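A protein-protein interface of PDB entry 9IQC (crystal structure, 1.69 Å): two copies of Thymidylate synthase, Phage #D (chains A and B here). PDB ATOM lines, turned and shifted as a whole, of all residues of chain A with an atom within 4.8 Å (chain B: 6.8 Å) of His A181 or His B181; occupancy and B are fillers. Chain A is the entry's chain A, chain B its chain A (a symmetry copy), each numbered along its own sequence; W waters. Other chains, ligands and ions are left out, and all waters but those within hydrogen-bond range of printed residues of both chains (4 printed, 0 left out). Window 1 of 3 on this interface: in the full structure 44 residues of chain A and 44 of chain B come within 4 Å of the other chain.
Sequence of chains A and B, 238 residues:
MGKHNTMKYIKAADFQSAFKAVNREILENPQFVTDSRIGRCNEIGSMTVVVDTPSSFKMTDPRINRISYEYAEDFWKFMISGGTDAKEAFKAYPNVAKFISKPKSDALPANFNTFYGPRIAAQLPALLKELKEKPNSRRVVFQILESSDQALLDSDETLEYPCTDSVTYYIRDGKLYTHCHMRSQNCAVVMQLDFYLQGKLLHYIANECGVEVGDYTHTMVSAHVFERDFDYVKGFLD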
ATOM      1  N   THR A 164     -31.332  13.265   1.229  1.00  0.00           N
ATOM      2  CA  THR A 164     -31.441  14.071   2.435  1.00  0.00           C
ATOM      3  C   THR A 164     -30.483  13.503   3.466  1.00  0.00           C
ATOM      4  O   THR A 164     -30.550  12.317   3.793  1.00  0.00           O
ATOM      5  CB  THR A 164     -32.884  14.039   2.953  1.00  0.00           C
ATOM      6  OG1 THR A 164     -33.764  14.475   1.910  1.00  0.00           O
ATOM      7  CG2 THR A 164     -33.048  14.930   4.178  1.00  0.00           C
ATOM      8  N   ASP A 165     -29.577  14.345   3.963  1.00  0.00           N
ATOM      9  CA  ASP A 165     -28.569  13.899   4.911  1.00  0.00           C
ATOM     10  C   ASP A 165     -29.117  13.937   6.342  1.00  0.00           C
ATOM     11  O   ASP A 165     -29.143  12.913   7.034  1.00  0.00           O
ATOM     12  CB  ASP A 165     -27.318  14.770   4.738  1.00  0.00           C
ATOM     13  CG  ASP A 165     -26.090  14.145   5.337  1.00  0.00           C
ATOM     14  OD1 ASP A 165     -26.176  12.982   5.775  1.00  0.00           O
ATOM     15  OD2 ASP A 165     -25.036  14.809   5.416  1.00  0.00           O
ATOM     16  N   SER A 166     -29.566  15.107   6.790  1.00  0.00           N
ATOM     17  CA  SER A 166     -30.126  15.228   8.129  1.00  0.00           C
ATOM     18  C   SER A 166     -31.047  16.437   8.183  1.00  0.00           C
ATOM     19  O   SER A 166     -30.997  17.322   7.325  1.00  0.00           O
ATOM     20  CB  SER A 166     -29.027  15.358   9.189  1.00  0.00           C
ATOM     21  OG  SER A 166     -28.348  16.583   9.012  1.00  0.00           O
ATOM     22  N   THR A 168     -32.158  19.143  11.248  1.00  0.00           N
ATOM     23  CA  THR A 168     -31.918  19.590  12.611  1.00  0.00           C
ATOM     24  C   THR A 168     -33.028  20.547  13.007  1.00  0.00           C
ATOM     25  O   THR A 168     -33.395  21.435  12.230  1.00  0.00           O
ATOM     26  CB  THR A 168     -30.562  20.285  12.749  1.00  0.00           C
ATOM     27  OG1 THR A 168     -29.534  19.416  12.268  1.00  0.00           O
ATOM     28  CG2 THR A 168     -30.288  20.603  14.229  1.00  0.00           C
ATOM     29  N   HIS A 179     -33.132  23.190  10.019  1.00  0.00           N
ATOM     30  CA  HIS A 179     -32.033  23.172   9.063  1.00  0.00           C
ATOM     31  C   HIS A 179     -32.000  21.808   8.390  1.00  0.00           C
ATOM     32  O   HIS A 179     -31.613  20.812   9.009  1.00  0.00           O
ATOM     33  CB  HIS A 179     -30.690  23.473   9.724  1.00  0.00           C
ATOM     34  CG  HIS A 179     -29.581  23.617   8.734  1.00  0.00           C
ATOM     35  ND1 HIS A 179     -28.827  24.766   8.623  1.00  0.00           N
ATOM     36  CD2 HIS A 179     -29.140  22.781   7.763  1.00  0.00           C
ATOM     37  CE1 HIS A 179     -27.952  24.622   7.644  1.00  0.00           C
ATOM     38  NE2 HIS A 179     -28.122  23.425   7.106  1.00  0.00           N
ATOM     39  N   CYS A 180     -32.406  21.774   7.129  1.00  0.00           N
ATOM     40  CA  CYS A 180     -32.358  20.566   6.321  1.00  0.00           C
ATOM     41  C   CYS A 180     -31.069  20.570   5.515  1.00  0.00           C
ATOM     42  O   CYS A 180     -30.854  21.467   4.696  1.00  0.00           O
ATOM     43  CB  CYS A 180     -33.558  20.499   5.383  1.00  0.00           C
ATOM     44  SG  CYS A 180     -33.525  19.067   4.294  1.00  0.00           S
ATOM     45  N   HIS A 181     -30.221  19.581   5.749  1.00  0.00           N
ATOM     46  CA  HIS A 181     -28.965  19.439   5.013  1.00  0.00           C
ATOM     47  C   HIS A 181     -29.144  18.347   3.967  1.00  0.00           C
ATOM     48  O   HIS A 181     -29.312  17.172   4.311  1.00  0.00           O
ATOM     49  CB  HIS A 181     -27.808  19.109   5.947  1.00  0.00           C
ATOM     50  CG  HIS A 181     -26.476  19.067   5.255  1.00  0.00           C
ATOM     51  ND1 HIS A 181     -25.989  20.129   4.525  1.00  0.00           N
ATOM     52  CD2 HIS A 181     -25.544  18.088   5.168  1.00  0.00           C
ATOM     53  CE1 HIS A 181     -24.805  19.813   4.028  1.00  0.00           C
ATOM     54  NE2 HIS A 181     -24.508  18.582   4.410  1.00  0.00           N
ATOM     55  N   MET A 182     -29.107  18.741   2.697  1.00  0.00           N
ATOM     56  CA  MET A 182     -29.202  17.818   1.572  1.00  0.00           C
ATOM     57  C   MET A 182     -27.813  17.462   1.073  1.00  0.00           C
ATOM     58  O   MET A 182     -27.008  18.351   0.783  1.00  0.00           O
ATOM     59  CB  MET A 182     -29.994  18.431   0.419  1.00  0.00           C
ATOM     60  CG  MET A 182     -31.410  18.858   0.778  1.00  0.00           C
ATOM     61  SD  MET A 182     -32.467  17.467   1.226  1.00  0.00           S
ATOM     62  CE  MET A 182     -32.630  16.632  -0.357  1.00  0.00           C
ATOM     63  N   ARG A 183     -27.544  16.163   0.975  1.00  0.00           N
ATOM     64  CA  ARG A 183     -26.383  15.705   0.222  1.00  0.00           C
ATOM     65  C   ARG A 183     -26.512  16.091  -1.245  1.00  0.00           C
ATOM     66  O   ARG A 183     -25.558  16.582  -1.860  1.00  0.00           O
ATOM     67  CB  ARG A 183     -26.261  14.189   0.370  1.00  0.00           C
ATOM     68  CG  ARG A 183     -25.266  13.560  -0.592  1.00  0.00           C
ATOM     69  CD  ARG A 183     -25.375  12.028  -0.553  1.00  0.00           C
ATOM     70  NE  ARG A 183     -26.613  11.531  -1.147  1.00  0.00           N
ATOM     71  CZ  ARG A 183     -26.814  11.401  -2.451  1.00  0.00           C
ATOM     72  NH1 ARG A 183     -25.907  11.790  -3.335  1.00  0.00           N
ATOM     73  NH2 ARG A 183     -27.947  10.853  -2.880  1.00  0.00           N
ATOM     74  N   THR A 219     -29.566  23.529   3.137  1.00  0.00           N
ATOM     75  CA  THR A 219     -28.238  23.471   2.539  1.00  0.00           C
ATOM     76  C   THR A 219     -28.147  22.271   1.608  1.00  0.00           C
ATOM     77  O   THR A 219     -28.753  21.220   1.842  1.00  0.00           O
ATOM     78  CB  THR A 219     -27.134  23.418   3.600  1.00  0.00           C
ATOM     79  OG1 THR A 219     -27.447  22.430   4.590  1.00  0.00           O
ATOM     80  CG2 THR A 219     -26.997  24.761   4.286  1.00  0.00           C
ATOM     81  N   VAL A 221     -25.232  20.166  -0.658  1.00  0.00           N
ATOM     82  CA  VAL A 221     -23.845  20.015  -1.079  1.00  0.00           C
ATOM     83  C   VAL A 221     -23.756  20.041  -2.601  1.00  0.00           C
ATOM     84  O   VAL A 221     -22.885  20.699  -3.182  1.00  0.00           O
ATOM     85  CB  VAL A 221     -23.225  18.738  -0.498  1.00  0.00           C
ATOM     86  CG1 VAL A 221     -21.754  18.654  -0.958  1.00  0.00           C
ATOM     87  CG2 VAL A 221     -23.267  18.774   1.018  1.00  0.00           C
ATOM     88  N   SER B  46     -27.455  28.363  11.631  1.00  0.00           N
ATOM     89  CA  SER B  46     -27.227  28.023  10.230  1.00  0.00           C
ATOM     90  C   SER B  46     -26.270  29.004   9.549  1.00  0.00           C
ATOM     91  O   SER B  46     -26.589  29.632   8.542  1.00  0.00           O
ATOM     92  CB  SER B  46     -28.562  27.942   9.484  1.00  0.00           C
ATOM     93  OG  SER B  46     -29.367  26.923  10.046  1.00  0.00           O
ATOM     94  N   MET B  47     -25.075  29.131  10.121  1.00  0.00           N
ATOM     95  CA  MET B  47     -24.003  29.864   9.460  1.00  0.00           C
ATOM     96  C   MET B  47     -23.368  29.009   8.375  1.00  0.00           C
ATOM     97  O   MET B  47     -23.250  27.789   8.516  1.00  0.00           O
ATOM     98  CB  MET B  47     -22.913  30.271  10.449  1.00  0.00           C
ATOM     99  CG  MET B  47     -23.293  31.348  11.411  1.00  0.00           C
ATOM    100  SD  MET B  47     -21.826  32.103  12.142  1.00  0.00           S
ATOM    101  CE  MET B  47     -21.485  33.375  10.940  1.00  0.00           C
ATOM    102  N   VAL B 141     -20.283  10.758   1.432  1.00  0.00           N
ATOM    103  CA  VAL B 141     -20.600  11.453   2.673  1.00  0.00           C
ATOM    104  C   VAL B 141     -20.137  10.609   3.848  1.00  0.00           C
ATOM    105  O   VAL B 141     -20.678   9.519   4.082  1.00  0.00           O
ATOM    106  CB  VAL B 141     -22.105  11.740   2.810  1.00  0.00           C
ATOM    107  CG1 VAL B 141     -22.333  12.518   4.085  1.00  0.00           C
ATOM    108  CG2 VAL B 141     -22.618  12.513   1.615  1.00  0.00           C
ATOM    109  N   CYS B 163     -20.601  16.620  17.615  1.00  0.00           N
ATOM    110  CA  CYS B 163     -20.872  17.962  17.115  1.00  0.00           C
ATOM    111  C   CYS B 163     -20.802  18.018  15.602  1.00  0.00           C
ATOM    112  O   CYS B 163     -21.445  18.870  14.982  1.00  0.00           O
ATOM    113  CB  CYS B 163     -19.872  18.947  17.709  1.00  0.00           C
ATOM    114  SG  CYS B 163     -19.823  18.909  19.522  1.00  0.00           S
ATOM    115  N   THR B 164     -19.997  17.146  15.004  1.00  0.00           N
ATOM    116  CA  THR B 164     -19.845  17.059  13.560  1.00  0.00           C
ATOM    117  C   THR B 164     -20.895  16.097  13.034  1.00  0.00           C
ATOM    118  O   THR B 164     -20.965  14.949  13.478  1.00  0.00           O
ATOM    119  CB  THR B 164     -18.434  16.573  13.212  1.00  0.00           C
ATOM    120  OG1 THR B 164     -17.476  17.447  13.824  1.00  0.00           O
ATOM    121  CG2 THR B 164     -18.219  16.538  11.704  1.00  0.00           C
ATOM    122  N   ASP B 165     -21.722  16.569  12.103  1.00  0.00           N
ATOM    123  CA  ASP B 165     -22.805  15.757  11.570  1.00  0.00           C
ATOM    124  C   ASP B 165     -22.308  14.881  10.418  1.00  0.00           C
ATOM    125  O   ASP B 165     -22.414  13.650  10.470  1.00  0.00           O
ATOM    126  CB  ASP B 165     -23.949  16.689  11.148  1.00  0.00           C
ATOM    127  CG  ASP B 165     -25.257  15.966  10.995  1.00  0.00           C
ATOM    128  OD1 ASP B 165     -25.310  14.768  11.338  1.00  0.00           O
ATOM    129  OD2 ASP B 165     -26.236  16.560  10.499  1.00  0.00           O
ATOM    130  N   SER B 166     -21.752  15.498   9.377  1.00  0.00           N
ATOM    131  CA  SER B 166     -21.230  14.741   8.249  1.00  0.00           C
ATOM    132  C   SER B 166     -20.189  15.575   7.520  1.00  0.00           C
ATOM    133  O   SER B 166     -20.113  16.796   7.683  1.00  0.00           O
ATOM    134  CB  SER B 166     -22.347  14.332   7.282  1.00  0.00           C
ATOM    135  OG  SER B 166     -22.883  15.487   6.672  1.00  0.00           O
ATOM    136  N   VAL B 167     -19.384  14.890   6.709  1.00  0.00           N
ATOM    137  CA  VAL B 167     -18.403  15.532   5.845  1.00  0.00           C
ATOM    138  C   VAL B 167     -18.583  14.945   4.456  1.00  0.00           C
ATOM    139  O   VAL B 167     -18.459  13.727   4.274  1.00  0.00           O
ATOM    140  CB  VAL B 167     -16.963  15.317   6.339  1.00  0.00           C
ATOM    141  CG1 VAL B 167     -15.992  16.128   5.485  1.00  0.00           C
ATOM    142  CG2 VAL B 167     -16.835  15.699   7.805  1.00  0.00           C
ATOM    143  N   THR B 168     -18.904  15.793   3.489  1.00  0.00           N
ATOM    144  CA  THR B 168     -19.142  15.367   2.119  1.00  0.00           C
ATOM    145  C   THR B 168     -17.951  15.777   1.272  1.00  0.00           C
ATOM    146  O   THR B 168     -17.465  16.907   1.382  1.00  0.00           O
ATOM    147  CB  THR B 168     -20.421  15.983   1.547  1.00  0.00           C
ATOM    148  OG1 THR B 168     -21.517  15.685   2.415  1.00  0.00           O
ATOM    149  CG2 THR B 168     -20.711  15.388   0.159  1.00  0.00           C
ATOM    150  N   HIS B 179     -17.461  19.648   2.107  1.00  0.00           N
ATOM    151  CA  HIS B 179     -18.521  20.318   2.849  1.00  0.00           C
ATOM    152  C   HIS B 179     -18.676  19.634   4.197  1.00  0.00           C
ATOM    153  O   HIS B 179     -19.189  18.513   4.278  1.00  0.00           O
ATOM    154  CB  HIS B 179     -19.847  20.309   2.090  1.00  0.00           C
ATOM    155  CG  HIS B 179     -20.899  21.129   2.762  1.00  0.00           C
ATOM    156  ND1 HIS B 179     -21.522  22.192   2.142  1.00  0.00           N
ATOM    157  CD2 HIS B 179     -21.392  21.086   4.023  1.00  0.00           C
ATOM    158  CE1 HIS B 179     -22.373  22.752   2.983  1.00  0.00           C
ATOM    159  NE2 HIS B 179     -22.312  22.098   4.133  1.00  0.00           N
ATOM    160  N   CYS B 180     -18.231  20.312   5.246  1.00  0.00           N
ATOM    161  CA  CYS B 180     -18.379  19.833   6.611  1.00  0.00           C
ATOM    162  C   CYS B 180     -19.632  20.453   7.212  1.00  0.00           C
ATOM    163  O   CYS B 180     -19.723  21.678   7.329  1.00  0.00           O
ATOM    164  CB  CYS B 180     -17.161  20.210   7.446  1.00  0.00           C
ATOM    165  SG  CYS B 180     -17.308  19.718   9.172  1.00  0.00           S
ATOM    166  N   HIS B 181     -20.588  19.615   7.581  1.00  0.00           N
ATOM    167  CA  HIS B 181     -21.825  20.073   8.213  1.00  0.00           C
ATOM    168  C   HIS B 181     -21.727  19.804   9.708  1.00  0.00           C
ATOM    169  O   HIS B 181     -21.698  18.645  10.135  1.00  0.00           O
ATOM    170  CB  HIS B 181     -23.044  19.378   7.616  1.00  0.00           C
ATOM    171  CG  HIS B 181     -24.348  19.898   8.151  1.00  0.00           C
ATOM    172  ND1 HIS B 181     -24.692  21.230   8.089  1.00  0.00           N
ATOM    173  CD2 HIS B 181     -25.374  19.268   8.769  1.00  0.00           C
ATOM    174  CE1 HIS B 181     -25.885  21.400   8.634  1.00  0.00           C
ATOM    175  NE2 HIS B 181     -26.324  20.223   9.049  1.00  0.00           N
ATOM    176  N   MET B 182     -21.677  20.876  10.494  1.00  0.00           N
ATOM    177  CA  MET B 182     -21.641  20.800  11.948  1.00  0.00           C
ATOM    178  C   MET B 182     -23.042  20.960  12.513  1.00  0.00           C
ATOM    179  O   MET B 182     -23.737  21.926  12.190  1.00  0.00           O
ATOM    180  CB  MET B 182     -20.748  21.888  12.540  1.00  0.00           C
ATOM    181  CG  MET B 182     -19.309  21.865  12.048  1.00  0.00           C
ATOM    182  SD  MET B 182     -18.422  20.377  12.551  1.00  0.00           S
ATOM    183  CE  MET B 182     -18.294  20.634  14.324  1.00  0.00           C
ATOM    184  N   ARG B 183     -23.444  20.010  13.353  1.00  0.00           N
ATOM    185  CA  ARG B 183     -24.620  20.215  14.189  1.00  0.00           C
ATOM    186  C   ARG B 183     -24.400  21.381  15.144  1.00  0.00           C
ATOM    187  O   ARG B 183     -25.273  22.240  15.313  1.00  0.00           O
ATOM    188  CB  ARG B 183     -24.908  18.933  14.967  1.00  0.00           C
ATOM    189  CG  ARG B 183     -25.930  19.107  16.079  1.00  0.00           C
ATOM    190  CD  ARG B 183     -25.986  17.852  16.962  1.00  0.00           C
ATOM    191  NE  ARG B 183     -24.788  17.676  17.777  1.00  0.00           N
ATOM    192  CZ  ARG B 183     -24.556  18.325  18.909  1.00  0.00           C
ATOM    193  NH1 ARG B 183     -25.385  19.258  19.357  1.00  0.00           N
ATOM    194  NH2 ARG B 183     -23.474  18.022  19.621  1.00  0.00           N
ATOM    195  N   SER B 184     -23.222  21.439  15.763  1.00  0.00           N
ATOM    196  CA  SER B 184     -23.006  22.355  16.872  1.00  0.00           C
ATOM    197  C   SER B 184     -21.537  22.735  16.875  1.00  0.00           C
ATOM    198  O   SER B 184     -20.684  21.850  16.810  1.00  0.00           O
ATOM    199  CB  SER B 184     -23.405  21.679  18.189  1.00  0.00           C
ATOM    200  OG  SER B 184     -23.091  22.484  19.308  1.00  0.00           O
ATOM    201  N   TYR B 216     -13.363  24.730   0.763  1.00  0.00           N
ATOM    202  CA  TYR B 216     -13.905  24.080   1.947  1.00  0.00           C
ATOM    203  C   TYR B 216     -15.108  24.869   2.432  1.00  0.00           C
ATOM    204  O   TYR B 216     -15.015  26.085   2.616  1.00  0.00           O
ATOM    205  CB  TYR B 216     -12.844  24.013   3.047  1.00  0.00           C
ATOM    206  CG  TYR B 216     -13.344  23.481   4.368  1.00  0.00           C
ATOM    207  CD1 TYR B 216     -13.438  22.111   4.590  1.00  0.00           C
ATOM    208  CD2 TYR B 216     -13.695  24.343   5.408  1.00  0.00           C
ATOM    209  CE1 TYR B 216     -13.880  21.606   5.801  1.00  0.00           C
ATOM    210  CE2 TYR B 216     -14.145  23.845   6.634  1.00  0.00           C
ATOM    211  CZ  TYR B 216     -14.233  22.475   6.819  1.00  0.00           C
ATOM    212  OH  TYR B 216     -14.655  21.954   8.016  1.00  0.00           O
ATOM    213  N   THR B 217     -16.226  24.184   2.641  1.00  0.00           N
ATOM    214  CA  THR B 217     -17.430  24.814   3.155  1.00  0.00           C
ATOM    215  C   THR B 217     -17.776  24.191   4.496  1.00  0.00           C
ATOM    216  O   THR B 217     -17.703  22.969   4.667  1.00  0.00           O
ATOM    217  CB  THR B 217     -18.591  24.684   2.170  1.00  0.00           C
ATOM    218  OG1 THR B 217     -18.197  25.259   0.922  1.00  0.00           O
ATOM    219  CG2 THR B 217     -19.829  25.426   2.684  1.00  0.00           C
ATOM    220  N   HIS B 218     -18.166  25.048   5.434  1.00  0.00           N
ATOM    221  CA  HIS B 218     -18.355  24.687   6.832  1.00  0.00           C
ATOM    222  C   HIS B 218     -19.720  25.248   7.204  1.00  0.00           C
ATOM    223  O   HIS B 218     -19.858  26.466   7.349  1.00  0.00           O
ATOM    224  CB  HIS B 218     -17.245  25.294   7.686  1.00  0.00           C
ATOM    225  CG  HIS B 218     -17.119  24.712   9.065  1.00  0.00           C
ATOM    226  ND1 HIS B 218     -16.445  23.533   9.318  1.00  0.00           N
ATOM    227  CD2 HIS B 218     -17.521  25.183  10.266  1.00  0.00           C
ATOM    228  CE1 HIS B 218     -16.460  23.292  10.617  1.00  0.00           C
ATOM    229  NE2 HIS B 218     -17.119  24.274  11.214  1.00  0.00           N
ATOM    230  N   THR B 219     -20.727  24.385   7.312  1.00  0.00           N
ATOM    231  CA  THR B 219     -22.032  24.835   7.781  1.00  0.00           C
ATOM    232  C   THR B 219     -22.218  24.441   9.238  1.00  0.00           C
ATOM    233  O   THR B 219     -21.736  23.399   9.696  1.00  0.00           O
ATOM    234  CB  THR B 219     -23.171  24.281   6.920  1.00  0.00           C
ATOM    235  OG1 THR B 219     -23.001  22.872   6.723  1.00  0.00           O
ATOM    236  CG2 THR B 219     -23.189  24.958   5.566  1.00  0.00           C
ATOM    237  N   MET B 220     -22.910  25.300   9.976  1.00  0.00           N
ATOM    238  CA  MET B 220     -23.060  25.109  11.414  1.00  0.00           C
ATOM    239  C   MET B 220     -24.502  25.423  11.770  1.00  0.00           C
ATOM    240  O   MET B 220     -24.923  26.574  11.657  1.00  0.00           O
ATOM    241  CB  MET B 220     -22.110  26.011  12.195  1.00  0.00           C
ATOM    242  CG  MET B 220     -20.621  25.752  11.917  1.00  0.00           C
ATOM    243  SD  MET B 220     -19.608  27.106  12.546  1.00  0.00           S
ATOM    244  CE  MET B 220     -19.899  28.362  11.326  1.00  0.00           C
ATOM    245  N   VAL B 221     -25.258  24.419  12.207  1.00  0.00           N
ATOM    246  CA  VAL B 221     -26.638  24.696  12.586  1.00  0.00           C
ATOM    247  C   VAL B 221     -26.670  25.630  13.791  1.00  0.00           C
ATOM    248  O   VAL B 221     -27.445  26.592  13.837  1.00  0.00           O
ATOM    249  CB  VAL B 221     -27.411  23.398  12.856  1.00  0.00           C
ATOM    250  CG1 VAL B 221     -28.864  23.762  13.223  1.00  0.00           C
ATOM    251  CG2 VAL B 221     -27.418  22.522  11.618  1.00  0.00           C
HETATM  252  O   HOH W   1     -26.778  18.713  12.255  1.00  0.00           O
HETATM  253  O   HOH W   2     -21.810  17.166   4.782  1.00  0.00           O
HETATM  254  O   HOH W   3     -24.331  15.426   2.746  1.00  0.00           O
HETATM  255  O   HOH W   4     -29.169  19.159   9.497  1.00  0.00           O
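Among the printed residues, pairs that only touch across the chains: Asp A165 with Val B141, Thr A168 with Val B221, His A179 with His B181, His A179 with Val B221, His A181 with His B179, His A181 with His B181, Arg A183 with Val B141, Val A221 with Thr B168 and Val A221 with His B179.
Asp A165 touches Ser B166, and with the chains exchanged Ser A166 touches Asp B165.
His A179 touches His B181, and with the chains exchanged His A181 touches His B179.
His A179 touches Val B221, and with the chains exchanged Val A221 touches His B179.
His B181 touches its own counterpart, His A181.
Positions printed for both chains: 164, 165, 166, 168, 179, 180, 181, 182, 183, 219 and 221.
Of the 12 pairs that touch across the chains among the printed residues, 9 have their exchanged pair printed and touching as well.
Thr A164 touches none of the printed residues of chain B.
Of the printed residues of chain B, Asp A165 touches Val B141 (3.8 Å) and Ser B166 (2.6 Å).
Printed residues of chain B within 4 Å of Ser A166: Asp B165 (2.6 Å).
Printed residues of chain B within 4 Å of His A179: Ser B46 (2.6 Å), His B181 (3.4 Å) and Val B221 (3.8 Å).
Of the printed residues of chain B, His A181 touches His B179 and His B181.
Of the printed residues of chain A, Ser B46 touches His A179 (2.6 Å).
Of the printed residues of chain A, Asp B165 touches Ser A166 (2.6 Å).
Of the printed residues of chain A, His B181 touches His A179 and His A181.
Arg B183 touches none of the printed residues of chain A.
The backbone NH of Asp A165 is in hydrogen-bond range of the backbone carbonyl oxygen of His A181, at 2.9 Å.
The backbone carbonyl oxygen of Met B182 sits at hydrogen-bond distance from the backbone NH of Val B221 (2.9 Å).
The backbone carbonyl oxygen (O) of Ser B166 is in hydrogen-bond range of the backbone NH (N) of His B181, 2.9 Å away.
The side-chain hydroxyl (OG1) of Thr B219 sits at hydrogen-bond distance from a ring nitrogen (NE2) of His B179 (2.8 Å).
A ring nitrogen (NE2) of His A179 is in hydrogen-bond range of the side-chain hydroxyl (OG1) of Thr A219, 2.8 Å away.
The backbone NH (N) of Asp B165 is in hydrogen-bond range of the backbone carbonyl oxygen (O) of His B181 (2.9 Å).
The side-chain hydroxyl of Ser A166 lies within hydrogen-bond range of the side-chain carboxylate of Asp B165, at 2.6 Å.
The side-chain hydroxyl (OG) of Ser B166 is in hydrogen-bond range of the side-chain carboxylate (OD2) of Asp A165, at 2.6 Å.
The side-chain hydroxyl (OG) of Ser B46 lies within hydrogen-bond range of a ring nitrogen (ND1) of His A179.
Water W4 lies within hydrogen-bond range of the side-chain hydroxyl (OG) of Ser A166 (2.7 Å), the side-chain hydroxyl (OG1) of Thr A168 (2.8 Å), the backbone carbonyl oxygen (O) of His A179 (3.0 Å) and a ring nitrogen (NE2) of His B181 (3.1 Å).
Water W2 lies within hydrogen-bond range of the side-chain hydroxyl (OG) of Ser B166 (2.7 Å), the side-chain hydroxyl (OG1) of Thr B168 (2.8 Å), the backbone carbonyl oxygen (O) of His B179 (3.0 Å) and a ring nitrogen (NE2) of His A181 (3.1 Å).
Water W3 lies within hydrogen-bond range of OD2 of Asp A165 (2.8 Å) and OG1 of Thr B168 (2.8 Å).
Water W1 lies within hydrogen-bond range of the side-chain carboxylate of Asp B165 (2.8 Å) and the side-chain hydroxyl of Thr A168 (2.8 Å).
Of the 21 printed residues of chain B, 8 touch a printed residue of chain A.
Hydrophobic or aromatic side chains of chain B that line the printed part of chain A: Val B141, His B179, His B181 and Val B221.
Along chain B the printed residues that touch a printed residue of chain A span positions 46 to 221.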
